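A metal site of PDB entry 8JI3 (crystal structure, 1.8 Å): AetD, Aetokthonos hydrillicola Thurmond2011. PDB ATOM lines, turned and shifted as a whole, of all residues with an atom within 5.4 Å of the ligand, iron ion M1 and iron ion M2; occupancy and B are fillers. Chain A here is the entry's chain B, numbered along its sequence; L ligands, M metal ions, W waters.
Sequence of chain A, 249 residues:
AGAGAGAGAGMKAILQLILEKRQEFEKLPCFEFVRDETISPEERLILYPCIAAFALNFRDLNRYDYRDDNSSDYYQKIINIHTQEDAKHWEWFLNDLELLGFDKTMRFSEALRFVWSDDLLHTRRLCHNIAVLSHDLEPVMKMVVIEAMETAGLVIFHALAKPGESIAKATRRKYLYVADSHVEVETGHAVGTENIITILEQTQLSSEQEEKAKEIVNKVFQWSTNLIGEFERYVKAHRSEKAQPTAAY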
ATOM      1  N   PHE A  25     -25.326  31.089  20.539  1.00  0.00           N
ATOM      2  CA  PHE A  25     -26.015  29.840  20.110  1.00  0.00           C
ATOM      3  C   PHE A  25     -27.506  29.918  20.438  1.00  0.00           C
ATOM      4  O   PHE A  25     -28.340  29.550  19.580  1.00  0.00           O
ATOM      5  CB  PHE A  25     -25.293  28.662  20.753  1.00  0.00           C
ATOM      6  CG  PHE A  25     -25.705  27.311  20.218  1.00  0.00           C
ATOM      7  CD1 PHE A  25     -25.442  26.962  18.912  1.00  0.00           C
ATOM      8  CD2 PHE A  25     -26.254  26.353  21.064  1.00  0.00           C
ATOM      9  CE1 PHE A  25     -25.792  25.707  18.437  1.00  0.00           C
ATOM     10  CE2 PHE A  25     -26.593  25.087  20.596  1.00  0.00           C
ATOM     11  CZ  PHE A  25     -26.349  24.765  19.291  1.00  0.00           C
ATOM     12  N   ILE A  51     -32.645  13.860  14.686  1.00  0.00           N
ATOM     13  CA  ILE A  51     -31.701  13.622  15.809  1.00  0.00           C
ATOM     14  C   ILE A  51     -31.251  12.148  15.717  1.00  0.00           C
ATOM     15  O   ILE A  51     -30.289  11.803  16.379  1.00  0.00           O
ATOM     16  CB  ILE A  51     -32.359  13.974  17.140  1.00  0.00           C
ATOM     17  CG1 ILE A  51     -32.682  15.475  17.162  1.00  0.00           C
ATOM     18  CG2 ILE A  51     -31.497  13.573  18.325  1.00  0.00           C
ATOM     19  CD1 ILE A  51     -33.516  15.879  18.354  1.00  0.00           C
ATOM     20  N   PHE A  54     -27.736  11.618  15.085  1.00  0.00           N
ATOM     21  CA  PHE A  54     -26.833  12.128  16.129  1.00  0.00           C
ATOM     22  C   PHE A  54     -26.920  11.239  17.391  1.00  0.00           C
ATOM     23  O   PHE A  54     -25.834  10.913  17.929  1.00  0.00           O
ATOM     24  CB  PHE A  54     -27.181  13.568  16.527  1.00  0.00           C
ATOM     25  CG  PHE A  54     -26.428  14.032  17.722  1.00  0.00           C
ATOM     26  CD1 PHE A  54     -25.157  14.582  17.616  1.00  0.00           C
ATOM     27  CD2 PHE A  54     -26.915  13.797  19.003  1.00  0.00           C
ATOM     28  CE1 PHE A  54     -24.417  14.918  18.738  1.00  0.00           C
ATOM     29  CE2 PHE A  54     -26.198  14.191  20.111  1.00  0.00           C
ATOM     30  CZ  PHE A  54     -24.950  14.730  19.983  1.00  0.00           C
ATOM     31  N   ALA A  55     -28.114  10.867  17.850  1.00  0.00           N
ATOM     32  CA  ALA A  55     -28.290  10.419  19.272  1.00  0.00           C
ATOM     33  C   ALA A  55     -27.487   9.137  19.549  1.00  0.00           C
ATOM     34  O   ALA A  55     -26.869   9.053  20.623  1.00  0.00           O
ATOM     35  CB  ALA A  55     -29.712  10.216  19.671  1.00  0.00           C
ATOM     36  N   PHE A  58     -23.735   9.651  19.491  1.00  0.00           N
ATOM     37  CA  PHE A  58     -23.355  10.341  20.711  1.00  0.00           C
ATOM     38  C   PHE A  58     -23.187   9.325  21.824  1.00  0.00           C
ATOM     39  O   PHE A  58     -22.222   9.436  22.587  1.00  0.00           O
ATOM     40  CB  PHE A  58     -24.405  11.401  21.078  1.00  0.00           C
ATOM     41  CG  PHE A  58     -24.004  12.182  22.288  1.00  0.00           C
ATOM     42  CD1 PHE A  58     -22.883  13.007  22.250  1.00  0.00           C
ATOM     43  CD2 PHE A  58     -24.677  12.037  23.489  1.00  0.00           C
ATOM     44  CE1 PHE A  58     -22.512  13.739  23.364  1.00  0.00           C
ATOM     45  CE2 PHE A  58     -24.286  12.780  24.601  1.00  0.00           C
ATOM     46  CZ  PHE A  58     -23.199  13.605  24.534  1.00  0.00           C
ATOM     47  N   HIS A  82     -19.433  11.026  34.164  1.00  0.00           N
ATOM     48  CA  HIS A  82     -20.255  11.917  33.298  1.00  0.00           C
ATOM     49  C   HIS A  82     -20.760  11.104  32.099  1.00  0.00           C
ATOM     50  O   HIS A  82     -21.969  11.080  31.833  1.00  0.00           O
ATOM     51  CB  HIS A  82     -19.386  13.128  32.929  1.00  0.00           C
ATOM     52  CG  HIS A  82     -20.049  14.228  32.186  1.00  0.00           C
ATOM     53  ND1 HIS A  82     -20.342  15.436  32.780  1.00  0.00           N
ATOM     54  CD2 HIS A  82     -20.387  14.346  30.878  1.00  0.00           C
ATOM     55  CE1 HIS A  82     -20.867  16.256  31.880  1.00  0.00           C
ATOM     56  NE2 HIS A  82     -20.918  15.591  30.704  1.00  0.00           N
ATOM     57  N   ASP A  86     -24.478  10.192  30.292  1.00  0.00           N
ATOM     58  CA  ASP A  86     -24.853  10.683  28.930  1.00  0.00           C
ATOM     59  C   ASP A  86     -25.081   9.489  27.987  1.00  0.00           C
ATOM     60  O   ASP A  86     -25.948   9.618  27.082  1.00  0.00           O
ATOM     61  CB  ASP A  86     -23.800  11.630  28.349  1.00  0.00           C
ATOM     62  CG  ASP A  86     -23.829  13.012  28.953  1.00  0.00           C
ATOM     63  OD1 ASP A  86     -24.902  13.492  29.222  1.00  0.00           O
ATOM     64  OD2 ASP A  86     -22.745  13.586  29.109  1.00  0.00           O
ATOM     65  N   HIS A  89     -28.953   8.228  27.357  1.00  0.00           N
ATOM     66  CA  HIS A  89     -30.004   9.145  26.843  1.00  0.00           C
ATOM     67  C   HIS A  89     -30.520   8.703  25.485  1.00  0.00           C
ATOM     68  O   HIS A  89     -31.717   8.971  25.155  1.00  0.00           O
ATOM     69  CB  HIS A  89     -29.509  10.598  26.893  1.00  0.00           C
ATOM     70  CG  HIS A  89     -29.161  11.077  28.260  1.00  0.00           C
ATOM     71  ND1 HIS A  89     -28.823  12.397  28.498  1.00  0.00           N
ATOM     72  CD2 HIS A  89     -29.181  10.445  29.457  1.00  0.00           C
ATOM     73  CE1 HIS A  89     -28.623  12.575  29.758  1.00  0.00           C
ATOM     74  NE2 HIS A  89     -28.846  11.373  30.415  1.00  0.00           N
ATOM     75  N   TRP A  90     -29.769   7.847  24.757  1.00  0.00           N
ATOM     76  CA  TRP A  90     -30.298   7.376  23.462  1.00  0.00           C
ATOM     77  C   TRP A  90     -31.604   6.606  23.637  1.00  0.00           C
ATOM     78  O   TRP A  90     -32.443   6.642  22.701  1.00  0.00           O
ATOM     79  CB  TRP A  90     -29.234   6.555  22.723  1.00  0.00           C
ATOM     80  CG  TRP A  90     -28.973   5.267  23.425  1.00  0.00           C
ATOM     81  CD1 TRP A  90     -28.233   5.111  24.557  1.00  0.00           C
ATOM     82  CD2 TRP A  90     -29.400   3.957  23.024  1.00  0.00           C
ATOM     83  NE1 TRP A  90     -28.194   3.783  24.887  1.00  0.00           N
ATOM     84  CE2 TRP A  90     -28.890   3.052  23.975  1.00  0.00           C
ATOM     85  CE3 TRP A  90     -30.133   3.440  21.942  1.00  0.00           C
ATOM     86  CZ2 TRP A  90     -29.094   1.667  23.883  1.00  0.00           C
ATOM     87  CZ3 TRP A  90     -30.344   2.076  21.851  1.00  0.00           C
ATOM     88  CH2 TRP A  90     -29.844   1.213  22.827  1.00  0.00           C
ATOM     89  N   LEU A 126     -20.987  15.228  13.506  1.00  0.00           N
ATOM     90  CA  LEU A 126     -20.590  16.028  14.678  1.00  0.00           C
ATOM     91  C   LEU A 126     -19.770  15.161  15.655  1.00  0.00           C
ATOM     92  O   LEU A 126     -18.657  15.578  16.050  1.00  0.00           O
ATOM     93  CB  LEU A 126     -21.857  16.596  15.332  1.00  0.00           C
ATOM     94  CG  LEU A 126     -21.607  17.379  16.626  1.00  0.00           C
ATOM     95  CD1 LEU A 126     -20.530  18.433  16.453  1.00  0.00           C
ATOM     96  CD2 LEU A 126     -22.878  17.998  17.120  1.00  0.00           C
ATOM     97  N   MET A 149     -19.610  20.949  24.398  1.00  0.00           N
ATOM     98  CA  MET A 149     -20.651  20.097  23.820  1.00  0.00           C
ATOM     99  C   MET A 149     -21.855  20.024  24.780  1.00  0.00           C
ATOM    100  O   MET A 149     -23.008  20.062  24.298  1.00  0.00           O
ATOM    101  CB  MET A 149     -20.052  18.707  23.577  1.00  0.00           C
ATOM    102  CG  MET A 149     -20.993  17.751  22.960  1.00  0.00           C
ATOM    103  SD  MET A 149     -21.428  18.335  21.313  1.00  0.00           S
ATOM    104  CE  MET A 149     -21.930  16.734  20.653  1.00  0.00           C
ATOM    105  N   GLU A 150     -21.605  19.848  26.072  1.00  0.00           N
ATOM    106  CA  GLU A 150     -22.698  19.720  27.074  1.00  0.00           C
ATOM    107  C   GLU A 150     -23.465  21.034  27.170  1.00  0.00           C
ATOM    108  O   GLU A 150     -24.702  20.976  27.296  1.00  0.00           O
ATOM    109  CB  GLU A 150     -22.171  19.336  28.445  1.00  0.00           C
ATOM    110  CG  GLU A 150     -21.681  17.908  28.484  1.00  0.00           C
ATOM    111  CD  GLU A 150     -22.777  16.877  28.310  1.00  0.00           C
ATOM    112  OE1 GLU A 150     -22.890  16.309  27.198  1.00  0.00           O
ATOM    113  OE2 GLU A 150     -23.484  16.630  29.285  1.00  0.00           O
ATOM    114  N   ALA A 152     -23.831  23.342  24.672  1.00  0.00           N
ATOM    115  CA  ALA A 152     -24.675  23.361  23.449  1.00  0.00           C
ATOM    116  C   ALA A 152     -25.852  22.421  23.619  1.00  0.00           C
ATOM    117  O   ALA A 152     -26.936  22.799  23.282  1.00  0.00           O
ATOM    118  CB  ALA A 152     -23.843  23.017  22.211  1.00  0.00           C
ATOM    119  N   GLY A 153     -25.634  21.209  24.124  1.00  0.00           N
ATOM    120  CA  GLY A 153     -26.719  20.257  24.421  1.00  0.00           C
ATOM    121  C   GLY A 153     -27.829  20.876  25.276  1.00  0.00           C
ATOM    122  O   GLY A 153     -29.029  20.655  24.992  1.00  0.00           O
ATOM    123  N   ILE A 156     -30.026  23.367  23.419  1.00  0.00           N
ATOM    124  CA  ILE A 156     -31.003  22.664  22.563  1.00  0.00           C
ATOM    125  C   ILE A 156     -32.130  22.081  23.389  1.00  0.00           C
ATOM    126  O   ILE A 156     -33.258  22.116  22.933  1.00  0.00           O
ATOM    127  CB  ILE A 156     -30.253  21.557  21.771  1.00  0.00           C
ATOM    128  CG1 ILE A 156     -29.306  22.198  20.750  1.00  0.00           C
ATOM    129  CG2 ILE A 156     -31.254  20.577  21.189  1.00  0.00           C
ATOM    130  CD1 ILE A 156     -28.232  21.245  20.191  1.00  0.00           C
ATOM    131  N   PHE A 157     -31.828  21.384  24.475  1.00  0.00           N
ATOM    132  CA  PHE A 157     -32.855  20.619  25.201  1.00  0.00           C
ATOM    133  C   PHE A 157     -33.714  21.574  26.058  1.00  0.00           C
ATOM    134  O   PHE A 157     -34.949  21.321  26.156  1.00  0.00           O
ATOM    135  CB  PHE A 157     -32.238  19.438  25.957  1.00  0.00           C
ATOM    136  CG  PHE A 157     -32.075  18.334  24.953  1.00  0.00           C
ATOM    137  CD1 PHE A 157     -33.134  17.517  24.586  1.00  0.00           C
ATOM    138  CD2 PHE A 157     -30.916  18.279  24.203  1.00  0.00           C
ATOM    139  CE1 PHE A 157     -32.962  16.565  23.586  1.00  0.00           C
ATOM    140  CE2 PHE A 157     -30.747  17.340  23.199  1.00  0.00           C
ATOM    141  CZ  PHE A 157     -31.806  16.512  22.873  1.00  0.00           C
ATOM    142  N   TYR A 177     -36.989  12.566  26.654  1.00  0.00           N
ATOM    143  CA  TYR A 177     -35.854  13.155  25.893  1.00  0.00           C
ATOM    144  C   TYR A 177     -36.089  14.655  25.725  1.00  0.00           C
ATOM    145  O   TYR A 177     -35.252  15.464  26.135  1.00  0.00           O
ATOM    146  CB  TYR A 177     -35.683  12.394  24.572  1.00  0.00           C
ATOM    147  CG  TYR A 177     -34.382  12.644  23.848  1.00  0.00           C
ATOM    148  CD1 TYR A 177     -33.161  12.308  24.389  1.00  0.00           C
ATOM    149  CD2 TYR A 177     -34.375  13.223  22.578  1.00  0.00           C
ATOM    150  CE1 TYR A 177     -31.964  12.477  23.717  1.00  0.00           C
ATOM    151  CE2 TYR A 177     -33.187  13.445  21.915  1.00  0.00           C
ATOM    152  CZ  TYR A 177     -31.968  13.098  22.473  1.00  0.00           C
ATOM    153  OH  TYR A 177     -30.807  13.363  21.821  1.00  0.00           O
ATOM    154  N   HIS A 182     -34.717  15.366  31.366  1.00  0.00           N
ATOM    155  CA  HIS A 182     -33.446  15.364  30.597  1.00  0.00           C
ATOM    156  C   HIS A 182     -32.683  16.680  30.816  1.00  0.00           C
ATOM    157  O   HIS A 182     -31.440  16.653  31.092  1.00  0.00           O
ATOM    158  CB  HIS A 182     -33.757  15.083  29.111  1.00  0.00           C
ATOM    159  CG  HIS A 182     -32.550  14.905  28.266  1.00  0.00           C
ATOM    160  ND1 HIS A 182     -32.610  14.914  26.885  1.00  0.00           N
ATOM    161  CD2 HIS A 182     -31.250  14.651  28.573  1.00  0.00           C
ATOM    162  CE1 HIS A 182     -31.405  14.789  26.410  1.00  0.00           C
ATOM    163  NE2 HIS A 182     -30.539  14.559  27.405  1.00  0.00           N
ATOM    164  N   VAL A 185     -30.813  16.649  34.122  1.00  0.00           N
ATOM    165  CA  VAL A 185     -29.523  15.911  34.083  1.00  0.00           C
ATOM    166  C   VAL A 185     -28.454  16.780  33.431  1.00  0.00           C
ATOM    167  O   VAL A 185     -27.316  16.820  33.984  1.00  0.00           O
ATOM    168  CB  VAL A 185     -29.673  14.546  33.378  1.00  0.00           C
ATOM    169  CG1 VAL A 185     -28.328  13.896  33.140  1.00  0.00           C
ATOM    170  CG2 VAL A 185     -30.585  13.627  34.191  1.00  0.00           C
ATOM    171  N   GLU A 186     -28.798  17.450  32.332  1.00  0.00           N
ATOM    172  CA  GLU A 186     -27.815  18.191  31.500  1.00  0.00           C
ATOM    173  C   GLU A 186     -27.407  19.465  32.236  1.00  0.00           C
ATOM    174  O   GLU A 186     -26.279  19.967  31.981  1.00  0.00           O
ATOM    175  CB  GLU A 186     -28.377  18.457  30.108  1.00  0.00           C
ATOM    176  CG  GLU A 186     -28.613  17.196  29.277  1.00  0.00           C
ATOM    177  CD  GLU A 186     -27.484  16.179  29.213  1.00  0.00           C
ATOM    178  OE1 GLU A 186     -26.340  16.502  29.601  1.00  0.00           O
ATOM    179  OE2 GLU A 186     -27.728  15.055  28.731  1.00  0.00           O
ATOM    180  N   HIS A 189     -24.608  18.640  34.283  1.00  0.00           N
ATOM    181  CA  HIS A 189     -23.425  18.376  33.392  1.00  0.00           C
ATOM    182  C   HIS A 189     -22.818  19.649  32.770  1.00  0.00           C
ATOM    183  O   HIS A 189     -21.623  19.603  32.415  1.00  0.00           O
ATOM    184  CB  HIS A 189     -23.812  17.424  32.255  1.00  0.00           C
ATOM    185  CG  HIS A 189     -24.044  16.010  32.679  1.00  0.00           C
ATOM    186  ND1 HIS A 189     -24.504  15.061  31.784  1.00  0.00           N
ATOM    187  CD2 HIS A 189     -23.891  15.389  33.876  1.00  0.00           C
ATOM    188  CE1 HIS A 189     -24.623  13.915  32.410  1.00  0.00           C
ATOM    189  NE2 HIS A 189     -24.229  14.073  33.699  1.00  0.00           N
ATOM    190  N   SER A 224     -21.835  22.554  16.103  1.00  0.00           N
ATOM    191  CA  SER A 224     -23.217  22.542  16.666  1.00  0.00           C
ATOM    192  C   SER A 224     -24.124  23.489  15.870  1.00  0.00           C
ATOM    193  O   SER A 224     -25.247  23.086  15.555  1.00  0.00           O
ATOM    194  CB  SER A 224     -23.211  22.857  18.114  1.00  0.00           C
ATOM    195  OG  SER A 224     -22.447  21.874  18.780  1.00  0.00           O
ATOM    196  N   LEU A 227     -25.151  21.858  12.642  1.00  0.00           N
ATOM    197  CA  LEU A 227     -26.194  20.850  12.897  1.00  0.00           C
ATOM    198  C   LEU A 227     -27.535  21.556  13.016  1.00  0.00           C
ATOM    199  O   LEU A 227     -28.563  21.139  12.407  1.00  0.00           O
ATOM    200  CB  LEU A 227     -25.717  20.107  14.151  1.00  0.00           C
ATOM    201  CG  LEU A 227     -26.708  19.137  14.762  1.00  0.00           C
ATOM    202  CD1 LEU A 227     -25.989  18.160  15.713  1.00  0.00           C
ATOM    203  CD2 LEU A 227     -27.731  19.907  15.583  1.00  0.00           C
ATOM    204  N   PHE A 231     -31.229  21.135  10.844  1.00  0.00           N
ATOM    205  CA  PHE A 231     -32.577  21.010  11.437  1.00  0.00           C
ATOM    206  C   PHE A 231     -33.454  22.115  10.831  1.00  0.00           C
ATOM    207  O   PHE A 231     -34.569  21.792  10.424  1.00  0.00           O
ATOM    208  CB  PHE A 231     -32.504  21.109  12.973  1.00  0.00           C
ATOM    209  CG  PHE A 231     -31.880  19.923  13.679  1.00  0.00           C
ATOM    210  CD1 PHE A 231     -31.277  18.885  12.967  1.00  0.00           C
ATOM    211  CD2 PHE A 231     -31.959  19.802  15.049  1.00  0.00           C
ATOM    212  CE1 PHE A 231     -30.724  17.781  13.618  1.00  0.00           C
ATOM    213  CE2 PHE A 231     -31.410  18.706  15.705  1.00  0.00           C
ATOM    214  CZ  PHE A 231     -30.781  17.695  14.991  1.00  0.00           C
HETATM  215  O1  LIG L   1     -28.489  12.995  23.186  1.00  0.00           O
HETATM  216  C1  LIG L   1     -28.470  13.590  24.324  1.00  0.00           C
HETATM  217  O2  LIG L   1     -28.837  13.023  25.388  1.00  0.00           O
HETATM  218  C2  LIG L   1     -28.015  15.091  24.386  1.00  0.00           C
HETATM  219  N1  LIG L   1     -28.250  15.666  25.734  1.00  0.00           N
HETATM  220  C3  LIG L   1     -26.557  15.331  24.040  1.00  0.00           C
HETATM  221  C4  LIG L   1     -26.075  16.532  23.148  1.00  0.00           C
HETATM  222  C5  LIG L   1     -26.564  17.015  21.990  1.00  0.00           C
HETATM  223  C6  LIG L   1     -27.585  16.686  21.163  1.00  0.00           C
HETATM  224  C7  LIG L   1     -27.791  17.344  19.898  1.00  0.00           C
HETATM  225 BR1  LIG L   1     -29.183  16.974  18.842  1.00  0.00          BR
HETATM  226  C8  LIG L   1     -26.909  18.341  19.610  1.00  0.00           C
HETATM  227  C9  LIG L   1     -25.880  18.629  20.448  1.00  0.00           C
HETATM  228 BR2  LIG L   1     -24.475  19.960  20.049  1.00  0.00          BR
HETATM  229  C10 LIG L   1     -25.727  17.996  21.624  1.00  0.00           C
HETATM  230  N2  LIG L   1     -24.758  18.115  22.465  1.00  0.00           N
HETATM  231  C11 LIG L   1     -25.004  17.236  23.480  1.00  0.00           C
HETATM  232 FE    FE M   1     -28.536  13.991  27.133  1.00  0.00          FE
HETATM  233 FE    FE M   2     -24.715  15.290  29.766  1.00  0.00          FE
HETATM  234  O   HOH W   1     -27.922  10.249  22.994  1.00  0.00           O
HETATM  235  O   HOH W   2     -26.458  13.534  27.086  1.00  0.00           O
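OE2 of Glu 150 lies close to NE2 of His 82. ND1 of His 182 is in hydrogen-bond range of O of Tyr 177 (2.8 Å). NE2 of His 82 lies close to OD2 of Asp 86, 3.1 Å away.
Iron ion M2 is bound by the side-chain carboxylate of Glu 150, the side-chain carboxylate of Asp 86, the side-chain carboxylate of Glu 186 and a ring nitrogen (ND1) of His 189. Slightly farther from iron ion M2 lies the side-chain carboxylate (OD2) of Asp 86 (2.7 Å).
Within 4 Å of iron ion M1: His 89, His 182 and Glu 186. The nearest printed residue that does not touch iron ion M1 is Asp 86 (4.2 Å).
His 82 touches iron ion M2 (NE2 to FE, 3.9 Å).
Iron ion M1 is bound by an oxygen (O2) of the ligand (2.0 Å), the side-chain carboxylate of Glu 186 (2.1 Å), a ring nitrogen (NE2) of His 182 (2.1 Å), a ring nitrogen (ND1) of His 89 (2.1 Å), water W2 (2.1 Å) and a nitrogen (N1) of the ligand (2.2 Å). Iron ion M1 has six donor atoms within binding distance.
O of Met 149 lies within hydrogen-bond range of N2 of the ligand (3.2 Å). The side-chain sulfur (SD) of Met 149 is in hydrogen-bond range of a nitrogen (N2) of the ligand (3.5 Å). An oxygen (O1) of the ligand is in hydrogen-bond range of the side-chain hydroxyl of Tyr 177, at 2.7 Å.
Merely in contact with the ligand: Phe 54 (3.0 Å), Phe 58 (3.5 Å), Leu 126 (3.9 Å), Ala 152 (3.8 Å), Gly 153 (3.5 Å), Ile 156 (3.2 Å), Phe 157 (3.7 Å) and Ser 224 (3.1 Å). Hydrophobic or aromatic side chains that line the ligand: Phe 54, Phe 58, His 89, Leu 126, Met 149, Ala 152, Ile 156, Phe 157, Tyr 177 and His 182. 13 residues have an atom within 4 Å of the ligand: Phe 54, Phe 58, His 89, Leu 126, Met 149, Ala 152, Gly 153, Ile 156, Phe 157, Tyr 177, His 182, Glu 186 and Ser 224.
Water W1 lies within hydrogen-bond range of an oxygen (O1) of the ligand (2.8 Å) and the backbone carbonyl oxygen (O) of Ala 55 (2.9 Å).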
